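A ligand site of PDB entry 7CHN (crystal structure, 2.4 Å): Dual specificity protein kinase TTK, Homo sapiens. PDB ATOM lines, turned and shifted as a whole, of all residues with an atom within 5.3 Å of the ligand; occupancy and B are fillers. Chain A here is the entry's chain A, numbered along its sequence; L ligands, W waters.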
ATOM      1  N   LYS A  15      -5.382  14.587   2.882  1.00  0.00           N
ATOM      2  CA  LYS A  15      -4.170  15.392   2.978  1.00  0.00           C
ATOM      3  C   LYS A  15      -3.270  14.739   4.010  1.00  0.00           C
ATOM      4  O   LYS A  15      -3.630  13.759   4.664  1.00  0.00           O
ATOM      5  CB  LYS A  15      -4.494  16.830   3.375  1.00  0.00           C
ATOM      6  CG  LYS A  15      -5.009  16.958   4.795  1.00  0.00           C
ATOM      7  CD  LYS A  15      -4.802  18.340   5.307  1.00  0.00           C
ATOM      8  CE  LYS A  15      -5.994  18.811   6.078  1.00  0.00           C
ATOM      9  NZ  LYS A  15      -5.803  20.250   6.404  1.00  0.00           N
ATOM     10  N   ILE A  17      -1.491  15.524   7.466  1.00  0.00           N
ATOM     11  CA  ILE A  17      -1.507  16.441   8.601  1.00  0.00           C
ATOM     12  C   ILE A  17      -0.092  16.782   9.031  1.00  0.00           C
ATOM     13  O   ILE A  17       0.248  17.953   9.228  1.00  0.00           O
ATOM     14  CB  ILE A  17      -2.310  15.826   9.769  1.00  0.00           C
ATOM     15  CG1 ILE A  17      -3.787  15.652   9.416  1.00  0.00           C
ATOM     16  CG2 ILE A  17      -2.105  16.649  11.033  1.00  0.00           C
ATOM     17  CD1 ILE A  17      -4.486  14.622  10.301  1.00  0.00           C
ATOM     18  N   GLY A  18       0.753  15.774   9.214  1.00  0.00           N
ATOM     19  CA  GLY A  18       2.032  16.059   9.820  1.00  0.00           C
ATOM     20  C   GLY A  18       3.036  14.955   9.585  1.00  0.00           C
ATOM     21  O   GLY A  18       2.753  13.922   8.973  1.00  0.00           O
ATOM     22  N   SER A  19       4.236  15.194  10.108  1.00  0.00           N
ATOM     23  CA  SER A  19       5.346  14.316   9.841  1.00  0.00           C
ATOM     24  C   SER A  19       6.381  14.565  10.921  1.00  0.00           C
ATOM     25  O   SER A  19       6.339  15.584  11.613  1.00  0.00           O
ATOM     26  CB  SER A  19       5.946  14.568   8.450  1.00  0.00           C
ATOM     27  OG  SER A  19       6.813  15.678   8.509  1.00  0.00           O
ATOM     28  N   VAL A  25       1.439  11.371   9.338  1.00  0.00           N
ATOM     29  CA  VAL A  25       0.043  11.247   9.711  1.00  0.00           C
ATOM     30  C   VAL A  25      -0.817  11.824   8.603  1.00  0.00           C
ATOM     31  O   VAL A  25      -0.552  12.930   8.113  1.00  0.00           O
ATOM     32  CB  VAL A  25      -0.260  11.939  11.052  1.00  0.00           C
ATOM     33  CG1 VAL A  25      -1.727  11.716  11.426  1.00  0.00           C
ATOM     34  CG2 VAL A  25       0.641  11.429  12.127  1.00  0.00           C
ATOM     35  N   GLN A  27      -4.909  12.597   7.133  1.00  0.00           N
ATOM     36  CA  GLN A  27      -6.358  12.638   7.237  1.00  0.00           C
ATOM     37  C   GLN A  27      -6.930  11.858   6.075  1.00  0.00           C
ATOM     38  O   GLN A  27      -6.508  12.048   4.930  1.00  0.00           O
ATOM     39  CB  GLN A  27      -6.845  14.093   7.235  1.00  0.00           C
ATOM     40  CG  GLN A  27      -8.341  14.282   7.290  1.00  0.00           C
ATOM     41  CD  GLN A  27      -8.723  15.765   7.202  1.00  0.00           C
ATOM     42  OE1 GLN A  27      -9.489  16.283   8.032  1.00  0.00           O
ATOM     43  NE2 GLN A  27      -8.167  16.459   6.217  1.00  0.00           N
ATOM     44  N   ALA A  37      -7.783   9.459  11.118  1.00  0.00           N
ATOM     45  CA  ALA A  37      -6.371   9.739  10.895  1.00  0.00           C
ATOM     46  C   ALA A  37      -5.613   8.418  10.809  1.00  0.00           C
ATOM     47  O   ALA A  37      -5.929   7.459  11.519  1.00  0.00           O
ATOM     48  CB  ALA A  37      -5.787  10.650  11.980  1.00  0.00           C
ATOM     49  N   LYS A  39      -1.603   7.104  10.995  1.00  0.00           N
ATOM     50  CA  LYS A  39      -0.175   7.316  11.185  1.00  0.00           C
ATOM     51  C   LYS A  39       0.607   6.216  10.470  1.00  0.00           C
ATOM     52  O   LYS A  39       0.308   5.026  10.607  1.00  0.00           O
ATOM     53  CB  LYS A  39       0.194   7.365  12.671  1.00  0.00           C
ATOM     54  CG  LYS A  39       1.634   7.840  12.946  1.00  0.00           C
ATOM     55  CD  LYS A  39       2.010   7.644  14.404  1.00  0.00           C
ATOM     56  CE  LYS A  39       2.622   8.903  14.992  1.00  0.00           C
ATOM     57  NZ  LYS A  39       3.733   8.693  15.970  1.00  0.00           N
ATOM     58  N   ILE A  72      -6.933   9.799  22.552  1.00  0.00           N
ATOM     59  CA  ILE A  72      -7.309   9.535  21.168  1.00  0.00           C
ATOM     60  C   ILE A  72      -7.351   8.024  20.948  1.00  0.00           C
ATOM     61  O   ILE A  72      -6.448   7.299  21.380  1.00  0.00           O
ATOM     62  CB  ILE A  72      -6.319  10.224  20.215  1.00  0.00           C
ATOM     63  CG1 ILE A  72      -6.553  11.729  20.199  1.00  0.00           C
ATOM     64  CG2 ILE A  72      -6.454   9.683  18.768  1.00  0.00           C
ATOM     65  CD1 ILE A  72      -7.718  12.177  19.284  1.00  0.00           C
ATOM     66  N   MET A  88      -6.686   5.885  13.569  1.00  0.00           N
ATOM     67  CA  MET A  88      -7.020   6.577  14.806  1.00  0.00           C
ATOM     68  C   MET A  88      -8.095   7.627  14.563  1.00  0.00           C
ATOM     69  O   MET A  88      -8.304   8.127  13.446  1.00  0.00           O
ATOM     70  CB  MET A  88      -5.789   7.257  15.436  1.00  0.00           C
ATOM     71  CG  MET A  88      -4.510   6.386  15.369  1.00  0.00           C
ATOM     72  SD  MET A  88      -3.150   7.219  16.193  1.00  0.00           S
ATOM     73  CE  MET A  88      -2.455   8.100  14.803  1.00  0.00           C
ATOM     74  N   GLU A  89      -8.761   7.938  15.666  1.00  0.00           N
ATOM     75  CA  GLU A  89      -9.578   9.124  15.768  1.00  0.00           C
ATOM     76  C   GLU A  89      -8.838  10.327  15.219  1.00  0.00           C
ATOM     77  O   GLU A  89      -7.650  10.556  15.490  1.00  0.00           O
ATOM     78  CB  GLU A  89      -9.959   9.341  17.244  1.00  0.00           C
ATOM     79  CG  GLU A  89     -11.235  10.115  17.528  1.00  0.00           C
ATOM     80  CD  GLU A  89     -11.451  10.317  19.027  1.00  0.00           C
ATOM     81  OE1 GLU A  89     -10.562   9.922  19.838  1.00  0.00           O
ATOM     82  OE2 GLU A  89     -12.503  10.852  19.404  1.00  0.00           O
ATOM     83  N   CYS A  90      -9.555  11.106  14.449  1.00  0.00           N
ATOM     84  CA  CYS A  90      -8.950  12.225  13.785  1.00  0.00           C
ATOM     85  C   CYS A  90      -9.394  13.480  14.529  1.00  0.00           C
ATOM     86  O   CYS A  90     -10.606  13.715  14.660  1.00  0.00           O
ATOM     87  CB  CYS A  90      -9.381  12.291  12.307  1.00  0.00           C
ATOM     88  SG  CYS A  90      -8.387  13.597  11.437  1.00  0.00           S
ATOM     89  N   GLY A  91      -8.453  14.286  14.996  1.00  0.00           N
ATOM     90  CA  GLY A  91      -8.810  15.562  15.590  1.00  0.00           C
ATOM     91  C   GLY A  91      -9.249  16.580  14.552  1.00  0.00           C
ATOM     92  O   GLY A  91      -8.992  16.436  13.356  1.00  0.00           O
ATOM     93  N   ASN A  92      -9.979  17.622  15.009  1.00  0.00           N
ATOM     94  CA  ASN A  92     -10.188  18.809  14.163  1.00  0.00           C
ATOM     95  C   ASN A  92      -8.876  19.557  13.937  1.00  0.00           C
ATOM     96  O   ASN A  92      -8.584  19.998  12.818  1.00  0.00           O
ATOM     97  CB  ASN A  92     -11.193  19.766  14.826  1.00  0.00           C
ATOM     98  CG  ASN A  92     -12.537  19.121  15.086  1.00  0.00           C
ATOM     99  OD1 ASN A  92     -12.752  17.944  14.791  1.00  0.00           O
ATOM    100  ND2 ASN A  92     -13.449  19.892  15.635  1.00  0.00           N
ATOM    101  N   ILE A  93      -8.049  19.651  14.977  1.00  0.00           N
ATOM    102  CA  ILE A  93      -6.841  20.469  14.947  1.00  0.00           C
ATOM    103  C   ILE A  93      -6.145  20.244  16.274  1.00  0.00           C
ATOM    104  O   ILE A  93      -6.778  19.812  17.237  1.00  0.00           O
ATOM    105  CB  ILE A  93      -7.174  21.956  14.725  1.00  0.00           C
ATOM    106  CG1 ILE A  93      -5.894  22.775  14.497  1.00  0.00           C
ATOM    107  CG2 ILE A  93      -7.954  22.512  15.929  1.00  0.00           C
ATOM    108  CD1 ILE A  93      -6.158  24.215  14.109  1.00  0.00           C
ATOM    109  N   ASP A  94      -4.855  20.530  16.353  1.00  0.00           N
ATOM    110  CA  ASP A  94      -4.200  20.419  17.639  1.00  0.00           C
ATOM    111  C   ASP A  94      -4.348  21.729  18.408  1.00  0.00           C
ATOM    112  O   ASP A  94      -4.529  22.803  17.841  1.00  0.00           O
ATOM    113  CB  ASP A  94      -2.731  20.058  17.458  1.00  0.00           C
ATOM    114  CG  ASP A  94      -1.955  21.143  16.806  1.00  0.00           C
ATOM    115  OD1 ASP A  94      -2.265  21.440  15.630  1.00  0.00           O
ATOM    116  OD2 ASP A  94      -1.027  21.695  17.448  1.00  0.00           O
ATOM    117  N   SER A  97      -1.907  24.661  17.388  1.00  0.00           N
ATOM    118  CA  SER A  97      -2.314  25.392  16.194  1.00  0.00           C
ATOM    119  C   SER A  97      -3.495  26.300  16.500  1.00  0.00           C
ATOM    120  O   SER A  97      -3.571  27.423  16.003  1.00  0.00           O
ATOM    121  CB  SER A  97      -2.701  24.403  15.089  1.00  0.00           C
ATOM    122  OG  SER A  97      -1.548  23.792  14.539  1.00  0.00           O
ATOM    123  N   ALA A 137       0.640  20.939  21.683  1.00  0.00           N
ATOM    124  CA  ALA A 137       0.619  20.016  20.555  1.00  0.00           C
ATOM    125  C   ALA A 137       0.180  18.603  20.937  1.00  0.00           C
ATOM    126  O   ALA A 137      -0.307  17.853  20.079  1.00  0.00           O
ATOM    127  CB  ALA A 137       1.997  19.950  19.887  1.00  0.00           C
ATOM    128  N   LEU A 140      -5.554  17.255  21.109  1.00  0.00           N
ATOM    129  CA  LEU A 140      -6.342  17.446  19.905  1.00  0.00           C
ATOM    130  C   LEU A 140      -7.746  17.883  20.285  1.00  0.00           C
ATOM    131  O   LEU A 140      -8.331  17.349  21.228  1.00  0.00           O
ATOM    132  CB  LEU A 140      -6.419  16.161  19.079  1.00  0.00           C
ATOM    133  CG  LEU A 140      -5.117  15.622  18.474  1.00  0.00           C
ATOM    134  CD1 LEU A 140      -5.378  14.390  17.565  1.00  0.00           C
ATOM    135  CD2 LEU A 140      -4.384  16.724  17.743  1.00  0.00           C
ATOM    136  N   ILE A 149      -2.772  12.884  22.603  1.00  0.00           N
ATOM    137  CA  ILE A 149      -2.278  12.072  21.496  1.00  0.00           C
ATOM    138  C   ILE A 149      -0.918  11.421  21.772  1.00  0.00           C
ATOM    139  O   ILE A 149      -0.660  10.343  21.239  1.00  0.00           O
ATOM    140  CB  ILE A 149      -2.242  12.878  20.167  1.00  0.00           C
ATOM    141  CG1 ILE A 149      -1.888  11.968  18.991  1.00  0.00           C
ATOM    142  CG2 ILE A 149      -1.226  13.997  20.206  1.00  0.00           C
ATOM    143  CD1 ILE A 149      -2.574  10.612  18.989  1.00  0.00           C
ATOM    144  N   MET A 157       5.928  14.544  16.299  1.00  0.00           N
ATOM    145  CA  MET A 157       5.777  15.039  14.942  1.00  0.00           C
ATOM    146  C   MET A 157       5.487  16.529  14.939  1.00  0.00           C
ATOM    147  O   MET A 157       5.298  17.155  15.984  1.00  0.00           O
ATOM    148  CB  MET A 157       4.669  14.285  14.213  1.00  0.00           C
ATOM    149  CG  MET A 157       4.480  12.866  14.658  1.00  0.00           C
ATOM    150  SD  MET A 157       3.704  12.054  13.271  1.00  0.00           S
ATOM    151  CE  MET A 157       5.095  12.026  12.162  1.00  0.00           C
ATOM    152  N   GLN A 158       5.424  17.115  13.750  1.00  0.00           N
ATOM    153  CA  GLN A 158       5.144  18.536  13.618  1.00  0.00           C
ATOM    154  C   GLN A 158       4.173  18.756  12.467  1.00  0.00           C
ATOM    155  O   GLN A 158       4.133  17.959  11.521  1.00  0.00           O
ATOM    156  CB  GLN A 158       6.448  19.337  13.417  1.00  0.00           C
ATOM    157  CG  GLN A 158       7.473  19.178  14.574  1.00  0.00           C
ATOM    158  CD  GLN A 158       7.500  20.364  15.548  1.00  0.00           C
ATOM    159  OE1 GLN A 158       7.096  20.242  16.709  1.00  0.00           O
ATOM    160  NE2 GLN A 158       7.990  21.509  15.080  1.00  0.00           N
ATOM    161  N   PRO A 159       3.360  19.812  12.552  1.00  0.00           N
ATOM    162  CA  PRO A 159       2.349  20.028  11.508  1.00  0.00           C
ATOM    163  C   PRO A 159       3.008  20.343  10.181  1.00  0.00           C
ATOM    164  O   PRO A 159       4.017  21.043  10.132  1.00  0.00           O
ATOM    165  CB  PRO A 159       1.523  21.222  12.005  1.00  0.00           C
ATOM    166  CG  PRO A 159       1.920  21.402  13.430  1.00  0.00           C
ATOM    167  CD  PRO A 159       3.320  20.875  13.575  1.00  0.00           C
ATOM    168  N   ASP A 160       2.445  19.801   9.108  1.00  0.00           N
ATOM    169  CA  ASP A 160       2.860  20.208   7.773  1.00  0.00           C
ATOM    170  C   ASP A 160       2.083  21.433   7.334  1.00  0.00           C
ATOM    171  O   ASP A 160       0.858  21.512   7.533  1.00  0.00           O
ATOM    172  CB  ASP A 160       2.630  19.095   6.748  1.00  0.00           C
ATOM    173  CG  ASP A 160       3.522  17.884   6.983  1.00  0.00           C
ATOM    174  OD1 ASP A 160       4.601  18.006   7.637  1.00  0.00           O
ATOM    175  OD2 ASP A 160       3.133  16.803   6.497  1.00  0.00           O
HETATM  176  C1  LIG L   1      -2.458  21.779  12.245  1.00  0.00           C
HETATM  177  C2  LIG L   1      -3.648  19.187  13.265  1.00  0.00           C
HETATM  178  C3  LIG L   1      -5.231  17.397  13.098  1.00  0.00           C
HETATM  179  C4  LIG L   1      -5.053  15.004  14.010  1.00  0.00           C
HETATM  180  C5  LIG L   1      -3.565  12.917  14.873  1.00  0.00           C
HETATM  181  C6  LIG L   1      -3.098  11.686  15.364  1.00  0.00           C
HETATM  182  N1  LIG L   1      -1.513  14.373  14.426  1.00  0.00           N
HETATM  183  C7  LIG L   1      -0.965  15.717  14.392  1.00  0.00           C
HETATM  184  C8  LIG L   1       1.288  16.930  13.857  1.00  0.00           C
HETATM  185  C9  LIG L   1       0.418  15.672  13.705  1.00  0.00           C
HETATM  186  C10 LIG L   1      -4.931  12.821  14.852  1.00  0.00           C
HETATM  187  C11 LIG L   1      -4.223  10.877  15.629  1.00  0.00           C
HETATM  188  C12 LIG L   1      -2.968  14.162  14.458  1.00  0.00           C
HETATM  189  C13 LIG L   1      -0.922  16.285  15.805  1.00  0.00           C
HETATM  190  C14 LIG L   1      -7.348  17.632  10.124  1.00  0.00           C
HETATM  191  C15 LIG L   1      -5.768  17.934  11.914  1.00  0.00           C
HETATM  192  C16 LIG L   1      -5.238  19.117  11.390  1.00  0.00           C
HETATM  193  C17 LIG L   1      -4.177  19.729  12.065  1.00  0.00           C
HETATM  194  C18 LIG L   1      -4.046  21.723  10.484  1.00  0.00           C
HETATM  195  C19 LIG L   1      -3.110  23.038  10.390  1.00  0.00           C
HETATM  196  C20 LIG L   1      -2.446  23.179  11.552  1.00  0.00           C
HETATM  197  C21 LIG L   1      -4.193  18.016  13.777  1.00  0.00           C
HETATM  198  C22 LIG L   1      -1.679  11.313  15.558  1.00  0.00           C
HETATM  199  C23 LIG L   1      -0.177  17.634  15.856  1.00  0.00           C
HETATM  200  C24 LIG L   1       1.243  17.539  15.262  1.00  0.00           C
HETATM  201  N2  LIG L   1      -3.623  20.990  11.570  1.00  0.00           N
HETATM  202  N3  LIG L   1      -5.863  16.134  13.551  1.00  0.00           N
HETATM  203  N4  LIG L   1      -5.648  13.907  14.409  1.00  0.00           N
HETATM  204  N5  LIG L   1      -0.605  11.038  15.707  1.00  0.00           N
HETATM  205  N6  LIG L   1      -5.311  11.571  15.313  1.00  0.00           N
HETATM  206  N7  LIG L   1      -3.753  15.149  14.038  1.00  0.00           N
HETATM  207  O1  LIG L   1      -6.801  17.215  11.350  1.00  0.00           O
HETATM  208  O2  LIG L   1      -4.913  21.443   9.733  1.00  0.00           O
HETATM  209  O   HOH W   1      -7.705  21.552  10.753  1.00  0.00           O
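N of Gly 91 is in hydrogen-bond range of N4 of the ligand, 2.9 Å away. The backbone carbonyl oxygen (O) of Gly 91 lies within hydrogen-bond range of a nitrogen (N3) of the ligand (3.1 Å). O of Glu 89 sits at hydrogen-bond distance from N6 of the ligand, at 2.6 Å.
OG of Ser 97 is in hydrogen-bond range of OD1 of Asp 94 (2.7 Å). The backbone NH (N) of Val 25 is in hydrogen-bond range of the backbone carbonyl oxygen (O) of Gly 18 (2.9 Å). The backbone NH of Gln 158 lies within hydrogen-bond range of the backbone carbonyl oxygen of Ser 19, at 2.8 Å. The backbone NH (N) of Gln 27 is in hydrogen-bond range of the backbone carbonyl oxygen (O) of Lys 15. The backbone carbonyl oxygen (O) of Val 25 sits at hydrogen-bond distance from the backbone NH (N) of Ile 17 (2.8 Å). N of Asp 160 sits at hydrogen-bond distance from O of Ile 17. N of Met 88 is in hydrogen-bond range of O of Ala 37 (2.7 Å).
Merely in contact with the ligand: Lys 15 (3.6 Å), Ile 17 (3.6 Å), Val 25 (3.8 Å), Gln 27 (3.3 Å), Ala 37 (3.5 Å), Lys 39 (3.9 Å), Met 88 (3.4 Å), Cys 90 (3.8 Å), Asn 92 (3.6 Å), Ile 93 (3.8 Å), Asp 94 (3.4 Å), Ser 97 (3.2 Å), Leu 140 (3.2 Å), Ile 149 (3.5 Å), Gln 158 (3.7 Å) and Pro 159 (3.8 Å). Hydrophobic or aromatic side chains within 4 Å of the ligand: Ile 17, Val 25, Ala 37, Met 88, Leu 140 and Ile 149. 18 residues have an atom within 4 Å of the ligand: Lys 15, Ile 17, Val 25, Gln 27, Ala 37, Lys 39, Met 88, Glu 89, Cys 90, Gly 91, Asn 92, Ile 93, Asp 94, Ser 97, Leu 140, Ile 149, Gln 158 and Pro 159.
Water W1 bridges O of Asn 92 (2.7 Å) and O2 of the ligand (3.0 Å).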
